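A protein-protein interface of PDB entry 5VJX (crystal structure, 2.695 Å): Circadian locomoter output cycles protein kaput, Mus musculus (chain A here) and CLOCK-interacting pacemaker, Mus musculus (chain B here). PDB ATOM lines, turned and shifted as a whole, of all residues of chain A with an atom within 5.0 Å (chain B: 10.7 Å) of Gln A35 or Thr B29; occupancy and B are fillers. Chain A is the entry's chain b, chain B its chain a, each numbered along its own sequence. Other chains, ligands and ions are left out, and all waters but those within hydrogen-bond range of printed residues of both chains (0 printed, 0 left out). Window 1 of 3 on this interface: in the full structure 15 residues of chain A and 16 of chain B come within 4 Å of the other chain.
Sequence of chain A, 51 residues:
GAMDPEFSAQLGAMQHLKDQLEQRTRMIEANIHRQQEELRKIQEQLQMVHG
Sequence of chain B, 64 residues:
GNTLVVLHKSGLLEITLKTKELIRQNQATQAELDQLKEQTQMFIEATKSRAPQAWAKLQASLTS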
ATOM      1  N   ILE A  28      -0.312 -17.082  -9.459  1.00  0.00           N
ATOM      2  CA  ILE A  28      -0.311 -15.651  -9.719  1.00  0.00           C
ATOM      3  C   ILE A  28       0.166 -14.883  -8.487  1.00  0.00           C
ATOM      4  O   ILE A  28       0.966 -13.966  -8.608  1.00  0.00           O
ATOM      5  CB  ILE A  28      -1.691 -15.145 -10.147  1.00  0.00           C
ATOM      6  CG1 ILE A  28      -2.065 -15.722 -11.509  1.00  0.00           C
ATOM      7  CG2 ILE A  28      -1.702 -13.634 -10.239  1.00  0.00           C
ATOM      8  CD1 ILE A  28      -3.468 -15.379 -11.932  1.00  0.00           C
ATOM      9  N   ASN A  31       3.797 -14.899  -8.365  1.00  0.00           N
ATOM     10  CA  ASN A  31       4.273 -14.019  -9.428  1.00  0.00           C
ATOM     11  C   ASN A  31       4.325 -12.567  -8.964  1.00  0.00           C
ATOM     12  O   ASN A  31       5.353 -11.883  -9.078  1.00  0.00           O
ATOM     13  CB  ASN A  31       3.355 -14.115 -10.650  1.00  0.00           C
ATOM     14  CG  ASN A  31       3.597 -15.357 -11.474  1.00  0.00           C
ATOM     15  OD1 ASN A  31       4.494 -16.143 -11.182  1.00  0.00           O
ATOM     16  ND2 ASN A  31       2.773 -15.557 -12.498  1.00  0.00           N
ATOM     17  N   ILE A  32       3.205 -12.112  -8.416  1.00  0.00           N
ATOM     18  CA  ILE A  32       3.089 -10.738  -7.964  1.00  0.00           C
ATOM     19  C   ILE A  32       4.105 -10.416  -6.874  1.00  0.00           C
ATOM     20  O   ILE A  32       4.732  -9.361  -6.913  1.00  0.00           O
ATOM     21  CB  ILE A  32       1.669 -10.431  -7.476  1.00  0.00           C
ATOM     22  CG1 ILE A  32       0.703 -10.452  -8.660  1.00  0.00           C
ATOM     23  CG2 ILE A  32       1.624  -9.083  -6.789  1.00  0.00           C
ATOM     24  CD1 ILE A  32      -0.700 -10.044  -8.323  1.00  0.00           C
ATOM     25  N   HIS A  33       4.314 -11.318  -5.920  1.00  0.00           N
ATOM     26  CA  HIS A  33       5.324 -11.006  -4.902  1.00  0.00           C
ATOM     27  C   HIS A  33       6.727 -10.873  -5.479  1.00  0.00           C
ATOM     28  O   HIS A  33       7.493  -9.986  -5.068  1.00  0.00           O
ATOM     29  CB  HIS A  33       5.315 -12.034  -3.784  1.00  0.00           C
ATOM     30  CG  HIS A  33       4.147 -11.892  -2.867  1.00  0.00           C
ATOM     31  ND1 HIS A  33       3.750 -12.886  -2.003  1.00  0.00           N
ATOM     32  CD2 HIS A  33       3.292 -10.862  -2.678  1.00  0.00           C
ATOM     33  CE1 HIS A  33       2.699 -12.474  -1.318  1.00  0.00           C
ATOM     34  NE2 HIS A  33       2.399 -11.250  -1.711  1.00  0.00           N
ATOM     35  N   ARG A  34       7.067 -11.741  -6.425  1.00  0.00           N
ATOM     36  CA  ARG A  34       8.372 -11.631  -7.062  1.00  0.00           C
ATOM     37  C   ARG A  34       8.485 -10.251  -7.708  1.00  0.00           C
ATOM     38  O   ARG A  34       9.511  -9.559  -7.554  1.00  0.00           O
ATOM     39  CB  ARG A  34       8.561 -12.735  -8.101  1.00  0.00           C
ATOM     40  CG  ARG A  34       9.913 -12.739  -8.791  1.00  0.00           C
ATOM     41  CD  ARG A  34      10.001 -13.834  -9.857  1.00  0.00           C
ATOM     42  NE  ARG A  34       8.999 -13.655 -10.908  1.00  0.00           N
ATOM     43  CZ  ARG A  34       7.912 -14.412 -11.055  1.00  0.00           C
ATOM     44  NH1 ARG A  34       7.680 -15.421 -10.223  1.00  0.00           N
ATOM     45  NH2 ARG A  34       7.056 -14.164 -12.041  1.00  0.00           N
ATOM     46  N   GLN A  35       7.399  -9.818  -8.358  1.00  0.00           N
ATOM     47  CA  GLN A  35       7.390  -8.504  -9.003  1.00  0.00           C
ATOM     48  C   GLN A  35       7.619  -7.403  -7.999  1.00  0.00           C
ATOM     49  O   GLN A  35       8.337  -6.454  -8.272  1.00  0.00           O
ATOM     50  CB  GLN A  35       6.055  -8.212  -9.695  1.00  0.00           C
ATOM     51  CG  GLN A  35       5.686  -9.065 -10.864  1.00  0.00           C
ATOM     52  CD  GLN A  35       4.314  -8.711 -11.385  1.00  0.00           C
ATOM     53  OE1 GLN A  35       3.553  -9.578 -11.803  1.00  0.00           O
ATOM     54  NE2 GLN A  35       3.986  -7.430 -11.353  1.00  0.00           N
ATOM     55  N   GLN A  36       7.003  -7.532  -6.834  1.00  0.00           N
ATOM     56  CA  GLN A  36       7.133  -6.529  -5.792  1.00  0.00           C
ATOM     57  C   GLN A  36       8.552  -6.431  -5.226  1.00  0.00           C
ATOM     58  O   GLN A  36       9.019  -5.336  -4.896  1.00  0.00           O
ATOM     59  CB  GLN A  36       6.113  -6.808  -4.694  1.00  0.00           C
ATOM     60  CG  GLN A  36       5.913  -5.666  -3.740  1.00  0.00           C
ATOM     61  CD  GLN A  36       4.838  -5.965  -2.730  1.00  0.00           C
ATOM     62  OE1 GLN A  36       4.287  -7.063  -2.701  1.00  0.00           O
ATOM     63  NE2 GLN A  36       4.549  -4.997  -1.875  1.00  0.00           N
ATOM     64  N   GLU A  37       9.257  -7.553  -5.121  1.00  0.00           N
ATOM     65  CA  GLU A  37      10.648  -7.446  -4.680  1.00  0.00           C
ATOM     66  C   GLU A  37      11.475  -6.784  -5.783  1.00  0.00           C
ATOM     67  O   GLU A  37      12.339  -5.948  -5.490  1.00  0.00           O
ATOM     68  CB  GLU A  37      11.247  -8.794  -4.273  1.00  0.00           C
ATOM     69  CG  GLU A  37      12.634  -8.670  -3.572  1.00  0.00           C
ATOM     70  CD  GLU A  37      12.630  -7.874  -2.253  1.00  0.00           C
ATOM     71  OE1 GLU A  37      11.606  -7.884  -1.529  1.00  0.00           O
ATOM     72  OE2 GLU A  37      13.661  -7.222  -1.948  1.00  0.00           O
ATOM     73  N   GLU A  38      11.245  -7.155  -7.045  1.00  0.00           N
ATOM     74  CA  GLU A  38      11.967  -6.468  -8.119  1.00  0.00           C
ATOM     75  C   GLU A  38      11.714  -4.964  -8.046  1.00  0.00           C
ATOM     76  O   GLU A  38      12.620  -4.158  -8.255  1.00  0.00           O
ATOM     77  CB  GLU A  38      11.601  -6.983  -9.507  1.00  0.00           C
ATOM     78  CG  GLU A  38      12.500  -6.338 -10.562  1.00  0.00           C
ATOM     79  CD  GLU A  38      12.430  -6.984 -11.927  1.00  0.00           C
ATOM     80  OE1 GLU A  38      11.719  -7.999 -12.071  1.00  0.00           O
ATOM     81  OE2 GLU A  38      13.079  -6.464 -12.864  1.00  0.00           O
ATOM     82  N   LEU A  39      10.474  -4.600  -7.758  1.00  0.00           N
ATOM     83  CA  LEU A  39      10.112  -3.213  -7.524  1.00  0.00           C
ATOM     84  C   LEU A  39      10.991  -2.584  -6.477  1.00  0.00           C
ATOM     85  O   LEU A  39      11.526  -1.501  -6.683  1.00  0.00           O
ATOM     86  CB  LEU A  39       8.668  -3.097  -7.074  1.00  0.00           C
ATOM     87  CG  LEU A  39       8.110  -1.680  -7.108  1.00  0.00           C
ATOM     88  CD1 LEU A  39       8.127  -1.121  -8.509  1.00  0.00           C
ATOM     89  CD2 LEU A  39       6.724  -1.654  -6.504  1.00  0.00           C
ATOM     90  N   LYS B  18      15.116  -2.347 -16.702  1.00  0.00           N
ATOM     91  CA  LYS B  18      14.490  -3.172 -15.669  1.00  0.00           C
ATOM     92  C   LYS B  18      13.056  -2.709 -15.416  1.00  0.00           C
ATOM     93  O   LYS B  18      12.188  -3.521 -15.141  1.00  0.00           O
ATOM     94  CB  LYS B  18      15.311  -3.190 -14.374  1.00  0.00           C
ATOM     95  CG  LYS B  18      16.630  -3.933 -14.538  1.00  0.00           C
ATOM     96  CD  LYS B  18      17.460  -4.066 -13.272  1.00  0.00           C
ATOM     97  CE  LYS B  18      16.770  -5.012 -12.296  1.00  0.00           C
ATOM     98  NZ  LYS B  18      16.668  -6.414 -12.807  1.00  0.00           N
ATOM     99  N   THR B  19      12.818  -1.400 -15.494  1.00  0.00           N
ATOM    100  CA  THR B  19      11.485  -0.833 -15.297  1.00  0.00           C
ATOM    101  C   THR B  19      10.530  -1.200 -16.442  1.00  0.00           C
ATOM    102  O   THR B  19       9.387  -1.549 -16.202  1.00  0.00           O
ATOM    103  CB  THR B  19      11.546   0.699 -15.144  1.00  0.00           C
ATOM    104  OG1 THR B  19      12.250   1.032 -13.947  1.00  0.00           O
ATOM    105  CG2 THR B  19      10.168   1.286 -15.053  1.00  0.00           C
ATOM    106  N   LYS B  20      10.986  -1.124 -17.688  1.00  0.00           N
ATOM    107  CA  LYS B  20      10.140  -1.538 -18.807  1.00  0.00           C
ATOM    108  C   LYS B  20       9.841  -3.028 -18.749  1.00  0.00           C
ATOM    109  O   LYS B  20       8.751  -3.465 -19.110  1.00  0.00           O
ATOM    110  CB  LYS B  20      10.766  -1.175 -20.149  1.00  0.00           C
ATOM    111  CG  LYS B  20      10.617   0.301 -20.500  1.00  0.00           C
ATOM    112  CD  LYS B  20      10.951   0.576 -21.957  1.00  0.00           C
ATOM    113  CE  LYS B  20      10.155   1.771 -22.467  1.00  0.00           C
ATOM    114  NZ  LYS B  20      10.423   2.049 -23.902  1.00  0.00           N
ATOM    115  N   GLU B  21      10.824  -3.804 -18.312  1.00  0.00           N
ATOM    116  CA  GLU B  21      10.662  -5.248 -18.148  1.00  0.00           C
ATOM    117  C   GLU B  21       9.654  -5.600 -17.038  1.00  0.00           C
ATOM    118  O   GLU B  21       8.850  -6.526 -17.174  1.00  0.00           O
ATOM    119  CB  GLU B  21      12.018  -5.892 -17.850  1.00  0.00           C
ATOM    120  CG  GLU B  21      12.020  -7.412 -17.849  1.00  0.00           C
ATOM    121  CD  GLU B  21      11.653  -8.003 -19.196  1.00  0.00           C
ATOM    122  OE1 GLU B  21      11.666  -7.270 -20.208  1.00  0.00           O
ATOM    123  OE2 GLU B  21      11.360  -9.214 -19.244  1.00  0.00           O
ATOM    124  N   LEU B  22       9.738  -4.883 -15.921  1.00  0.00           N
ATOM    125  CA  LEU B  22       8.812  -5.057 -14.807  1.00  0.00           C
ATOM    126  C   LEU B  22       7.396  -4.651 -15.168  1.00  0.00           C
ATOM    127  O   LEU B  22       6.436  -5.269 -14.717  1.00  0.00           O
ATOM    128  CB  LEU B  22       9.269  -4.259 -13.598  1.00  0.00           C
ATOM    129  CG  LEU B  22       8.368  -4.378 -12.372  1.00  0.00           C
ATOM    130  CD1 LEU B  22       8.183  -5.811 -11.952  1.00  0.00           C
ATOM    131  CD2 LEU B  22       8.919  -3.551 -11.242  1.00  0.00           C
ATOM    132  N   ILE B  23       7.278  -3.589 -15.959  1.00  0.00           N
ATOM    133  CA  ILE B  23       5.998  -3.159 -16.499  1.00  0.00           C
ATOM    134  C   ILE B  23       5.405  -4.231 -17.403  1.00  0.00           C
ATOM    135  O   ILE B  23       4.217  -4.538 -17.339  1.00  0.00           O
ATOM    136  CB  ILE B  23       6.142  -1.857 -17.281  1.00  0.00           C
ATOM    137  CG1 ILE B  23       6.329  -0.694 -16.316  1.00  0.00           C
ATOM    138  CG2 ILE B  23       4.913  -1.609 -18.122  1.00  0.00           C
ATOM    139  CD1 ILE B  23       6.781   0.565 -16.953  1.00  0.00           C
ATOM    140  N   ARG B  24       6.254  -4.807 -18.236  1.00  0.00           N
ATOM    141  CA  ARG B  24       5.847  -5.868 -19.135  1.00  0.00           C
ATOM    142  C   ARG B  24       5.296  -7.055 -18.340  1.00  0.00           C
ATOM    143  O   ARG B  24       4.198  -7.564 -18.603  1.00  0.00           O
ATOM    144  CB  ARG B  24       7.038  -6.299 -19.980  1.00  0.00           C
ATOM    145  CG  ARG B  24       6.691  -7.152 -21.162  1.00  0.00           C
ATOM    146  CD  ARG B  24       7.905  -7.902 -21.673  1.00  0.00           C
ATOM    147  NE  ARG B  24       8.542  -8.683 -20.621  1.00  0.00           N
ATOM    148  CZ  ARG B  24       8.067  -9.838 -20.171  1.00  0.00           C
ATOM    149  NH1 ARG B  24       6.944 -10.329 -20.664  1.00  0.00           N
ATOM    150  NH2 ARG B  24       8.703 -10.495 -19.219  1.00  0.00           N
ATOM    151  N   GLN B  25       6.077  -7.489 -17.361  1.00  0.00           N
ATOM    152  CA  GLN B  25       5.703  -8.611 -16.514  1.00  0.00           C
ATOM    153  C   GLN B  25       4.392  -8.338 -15.785  1.00  0.00           C
ATOM    154  O   GLN B  25       3.529  -9.206 -15.682  1.00  0.00           O
ATOM    155  CB  GLN B  25       6.826  -8.913 -15.522  1.00  0.00           C
ATOM    156  CG  GLN B  25       8.040  -9.546 -16.178  1.00  0.00           C
ATOM    157  CD  GLN B  25       9.150  -9.877 -15.201  1.00  0.00           C
ATOM    158  OE1 GLN B  25       9.124  -9.453 -14.043  1.00  0.00           O
ATOM    159  NE2 GLN B  25      10.142 -10.635 -15.670  1.00  0.00           N
ATOM    160  N   ASN B  26       4.251  -7.120 -15.284  1.00  0.00           N
ATOM    161  CA  ASN B  26       3.047  -6.720 -14.577  1.00  0.00           C
ATOM    162  C   ASN B  26       1.813  -6.718 -15.465  1.00  0.00           C
ATOM    163  O   ASN B  26       0.721  -7.049 -15.016  1.00  0.00           O
ATOM    164  CB  ASN B  26       3.243  -5.343 -13.968  1.00  0.00           C
ATOM    165  CG  ASN B  26       2.104  -4.939 -13.086  1.00  0.00           C
ATOM    166  OD1 ASN B  26       1.651  -5.713 -12.251  1.00  0.00           O
ATOM    167  ND2 ASN B  26       1.620  -3.716 -13.270  1.00  0.00           N
ATOM    168  N   GLN B  27       1.981  -6.340 -16.725  1.00  0.00           N
ATOM    169  CA  GLN B  27       0.868  -6.406 -17.663  1.00  0.00           C
ATOM    170  C   GLN B  27       0.479  -7.847 -17.948  1.00  0.00           C
ATOM    171  O   GLN B  27      -0.705  -8.161 -18.079  1.00  0.00           O
ATOM    172  CB  GLN B  27       1.199  -5.695 -18.964  1.00  0.00           C
ATOM    173  CG  GLN B  27       0.292  -4.519 -19.236  1.00  0.00           C
ATOM    174  CD  GLN B  27      -1.175  -4.855 -19.040  1.00  0.00           C
ATOM    175  OE1 GLN B  27      -1.858  -4.233 -18.228  1.00  0.00           O
ATOM    176  NE2 GLN B  27      -1.671  -5.833 -19.792  1.00  0.00           N
ATOM    177  N   ALA B  28       1.474  -8.721 -18.079  1.00  0.00           N
ATOM    178  CA  ALA B  28       1.195 -10.153 -18.212  1.00  0.00           C
ATOM    179  C   ALA B  28       0.415 -10.694 -17.005  1.00  0.00           C
ATOM    180  O   ALA B  28      -0.565 -11.420 -17.164  1.00  0.00           O
ATOM    181  CB  ALA B  28       2.479 -10.927 -18.402  1.00  0.00           C
ATOM    182  N   THR B  29       0.858 -10.353 -15.800  1.00  0.00           N
ATOM    183  CA  THR B  29       0.155 -10.789 -14.601  1.00  0.00           C
ATOM    184  C   THR B  29      -1.268 -10.242 -14.558  1.00  0.00           C
ATOM    185  O   THR B  29      -2.191 -10.936 -14.154  1.00  0.00           O
ATOM    186  CB  THR B  29       0.892 -10.362 -13.324  1.00  0.00           C
ATOM    187  OG1 THR B  29       2.061 -11.168 -13.151  1.00  0.00           O
ATOM    188  CG2 THR B  29       0.017 -10.534 -12.115  1.00  0.00           C
ATOM    189  N   GLN B  30      -1.452  -9.015 -15.025  1.00  0.00           N
ATOM    190  CA  GLN B  30      -2.789  -8.453 -15.128  1.00  0.00           C
ATOM    191  C   GLN B  30      -3.664  -9.243 -16.087  1.00  0.00           C
ATOM    192  O   GLN B  30      -4.840  -9.468 -15.815  1.00  0.00           O
ATOM    193  CB  GLN B  30      -2.724  -6.995 -15.578  1.00  0.00           C
ATOM    194  CG  GLN B  30      -4.080  -6.343 -15.771  1.00  0.00           C
ATOM    195  CD  GLN B  30      -4.878  -6.249 -14.504  1.00  0.00           C
ATOM    196  OE1 GLN B  30      -4.465  -5.613 -13.544  1.00  0.00           O
ATOM    197  NE2 GLN B  30      -6.027  -6.907 -14.485  1.00  0.00           N
ATOM    198  N   ALA B  31      -3.105  -9.652 -17.217  1.00  0.00           N
ATOM    199  CA  ALA B  31      -3.872 -10.446 -18.166  1.00  0.00           C
ATOM    200  C   ALA B  31      -4.289 -11.784 -17.572  1.00  0.00           C
ATOM    201  O   ALA B  31      -5.472 -12.165 -17.616  1.00  0.00           O
ATOM    202  CB  ALA B  31      -3.075 -10.659 -19.435  1.00  0.00           C
ATOM    203  N   GLU B  32      -3.318 -12.487 -16.994  1.00  0.00           N
ATOM    204  CA  GLU B  32      -3.607 -13.760 -16.343  1.00  0.00           C
ATOM    205  C   GLU B  32      -4.678 -13.586 -15.275  1.00  0.00           C
ATOM    206  O   GLU B  32      -5.581 -14.412 -15.138  1.00  0.00           O
ATOM    207  CB  GLU B  32      -2.347 -14.379 -15.745  1.00  0.00           C
ATOM    208  CG  GLU B  32      -2.514 -15.856 -15.450  1.00  0.00           C
ATOM    209  CD  GLU B  32      -1.262 -16.503 -14.913  1.00  0.00           C
ATOM    210  OE1 GLU B  32      -0.177 -15.879 -14.993  1.00  0.00           O
ATOM    211  OE2 GLU B  32      -1.373 -17.640 -14.406  1.00  0.00           O
ATOM    212  N   LEU B  33      -4.576 -12.503 -14.521  1.00  0.00           N
ATOM    213  CA  LEU B  33      -5.512 -12.229 -13.439  1.00  0.00           C
ATOM    214  C   LEU B  33      -6.917 -11.970 -13.958  1.00  0.00           C
ATOM    215  O   LEU B  33      -7.887 -12.418 -13.362  1.00  0.00           O
ATOM    216  CB  LEU B  33      -5.021 -11.039 -12.617  1.00  0.00           C
ATOM    217  CG  LEU B  33      -5.765 -10.709 -11.337  1.00  0.00           C
ATOM    218  CD1 LEU B  33      -5.938 -11.951 -10.524  1.00  0.00           C
ATOM    219  CD2 LEU B  33      -4.959  -9.691 -10.574  1.00  0.00           C
ATOM    220  N   ASP B  34      -7.028 -11.254 -15.073  1.00  0.00           N
ATOM    221  CA  ASP B  34      -8.333 -11.014 -15.678  1.00  0.00           C
ATOM    222  C   ASP B  34      -8.983 -12.313 -16.155  1.00  0.00           C
ATOM    223  O   ASP B  34     -10.180 -12.527 -15.942  1.00  0.00           O
ATOM    224  CB  ASP B  34      -8.227 -10.013 -16.830  1.00  0.00           C
ATOM    225  CG  ASP B  34      -7.925  -8.606 -16.350  1.00  0.00           C
ATOM    226  OD1 ASP B  34      -8.205  -8.309 -15.171  1.00  0.00           O
ATOM    227  OD2 ASP B  34      -7.433  -7.790 -17.153  1.00  0.00           O
ATOM    228  N   GLN B  35      -8.208 -13.171 -16.815  1.00  0.00           N
ATOM    229  CA  GLN B  35      -8.764 -14.458 -17.251  1.00  0.00           C
ATOM    230  C   GLN B  35      -9.189 -15.354 -16.086  1.00  0.00           C
ATOM    231  O   GLN B  35     -10.260 -15.980 -16.107  1.00  0.00           O
ATOM    232  CB  GLN B  35      -7.777 -15.221 -18.127  1.00  0.00           C
ATOM    233  CG  GLN B  35      -8.420 -16.426 -18.786  1.00  0.00           C
ATOM    234  CD  GLN B  35      -7.533 -17.077 -19.814  1.00  0.00           C
ATOM    235  OE1 GLN B  35      -6.421 -16.619 -20.070  1.00  0.00           O
ATOM    236  NE2 GLN B  35      -8.009 -18.171 -20.395  1.00  0.00           N
ATOM    237  N   LEU B  36      -8.337 -15.431 -15.071  1.00  0.00           N
ATOM    238  CA  LEU B  36      -8.660 -16.230 -13.904  1.00  0.00           C
ATOM    239  C   LEU B  36      -9.923 -15.659 -13.268  1.00  0.00           C
ATOM    240  O   LEU B  36     -10.754 -16.397 -12.745  1.00  0.00           O
ATOM    241  CB  LEU B  36      -7.505 -16.236 -12.909  1.00  0.00           C
ATOM    242  CG  LEU B  36      -7.721 -17.003 -11.609  1.00  0.00           C
ATOM    243  CD1 LEU B  36      -7.832 -18.476 -11.911  1.00  0.00           C
ATOM    244  CD2 LEU B  36      -6.579 -16.737 -10.665  1.00  0.00           C
ATOM    245  N   LYS B  37     -10.066 -14.337 -13.338  1.00  0.00           N
ATOM    246  CA  LYS B  37     -11.250 -13.669 -12.812  1.00  0.00           C
ATOM    247  C   LYS B  37     -12.506 -14.056 -13.566  1.00  0.00           C
ATOM    248  O   LYS B  37     -13.535 -14.305 -12.960  1.00  0.00           O
ATOM    249  CB  LYS B  37     -11.105 -12.150 -12.873  1.00  0.00           C
ATOM    250  CG  LYS B  37     -12.360 -11.422 -12.411  1.00  0.00           C
ATOM    251  CD  LYS B  37     -12.254  -9.912 -12.531  1.00  0.00           C
ATOM    252  CE  LYS B  37     -13.607  -9.276 -12.256  1.00  0.00           C
ATOM    253  NZ  LYS B  37     -14.690 -10.052 -12.920  1.00  0.00           N
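The guanidinium group of Arg A34 is in hydrogen-bond range of the side-chain amide oxygen of Asn A31 (3.3 Å).
Of the 10 printed residues of chain A, 6 touch a printed residue of chain B.
Hydrophobic or aromatic side chains of chain A within 4 Å of the printed part of chain B: Ile A28, Ile A32 and Leu A39.
Along chain A the printed residues that touch a printed residue of chain B span positions 28 to 39.
Of the 20 printed residues of chain B, 7 touch a printed residue of chain A.
Printed residues of chain B that touch a printed residue of chain A: Lys B18, Leu B22, Gln B25, Asn B26, Thr B29, Glu B32 and Leu B36.
Hydrophobic or aromatic side chains of chain B within 4 Å of the printed part of chain A: Leu B22 and Leu B36.
Among the printed residues, 11 pairs touch across the chains.
Among the printed residues, Asp or Glu carboxylates within 4 Å of a Lys or Arg side-chain nitrogen of the other chain: Glu A38 with Lys B18.
OE2 of Glu B32 touches CG1 of Ile A28, 3.5 Å away.
Ile A28 touches Leu B36.
Glu B32 touches Asn A31 (OE1 to ND2, 3.9 Å).
Ile A32 touches Thr B29.
O of Gln A35 touches CD1 of Leu B22 (3.7 Å).
OE1 of Gln A35 touches O of Gln B25, at 3.9 Å.
Gln B25 touches Glu A38.
CD2 of Leu B22 touches CD1 of Leu A39, 3.7 Å away.
NZ of Lys B18 lies within salt-bridge range of OE2 of Glu A38, 3.6 Å away.
The side-chain amide oxygen (OD1) of Asn B26 lies within hydrogen-bond range of the side-chain amide nitrogen (NE2) of Gln A35, 3.0 Å away.
The side-chain hydroxyl of Thr B29 lies within hydrogen-bond range of the side-chain amide oxygen of Gln A35 (2.6 Å).
Of chain B, only Thr B29 comes within 4 Å of Ile A32.
His A33 touches none of the printed residues of chain B.
Printed residues of chain B within 4 Å of Glu A38: Lys B18 (3.6 Å) and Gln B25 (3.6 Å).
Of the printed residues of chain A, Lys B18 touches Glu A38.
Printed residues of chain A within 4 Å of Leu B22: Gln A35 (3.7 Å) and Leu A39 (3.7 Å).
Printed residues of chain A within 4 Å of Gln B25: Gln A35 (3.9 Å) and Glu A38 (3.6 Å).
Printed residues of chain A within 4 Å of Thr B29: Ile A32 and Gln A35.
The nearest residue of chain B that does not touch Gln A35 is Gln B27 (5.8 Å).
The nearest printed residue of chain A that does not touch Thr B29 is Ile A28 (4.01 Å).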
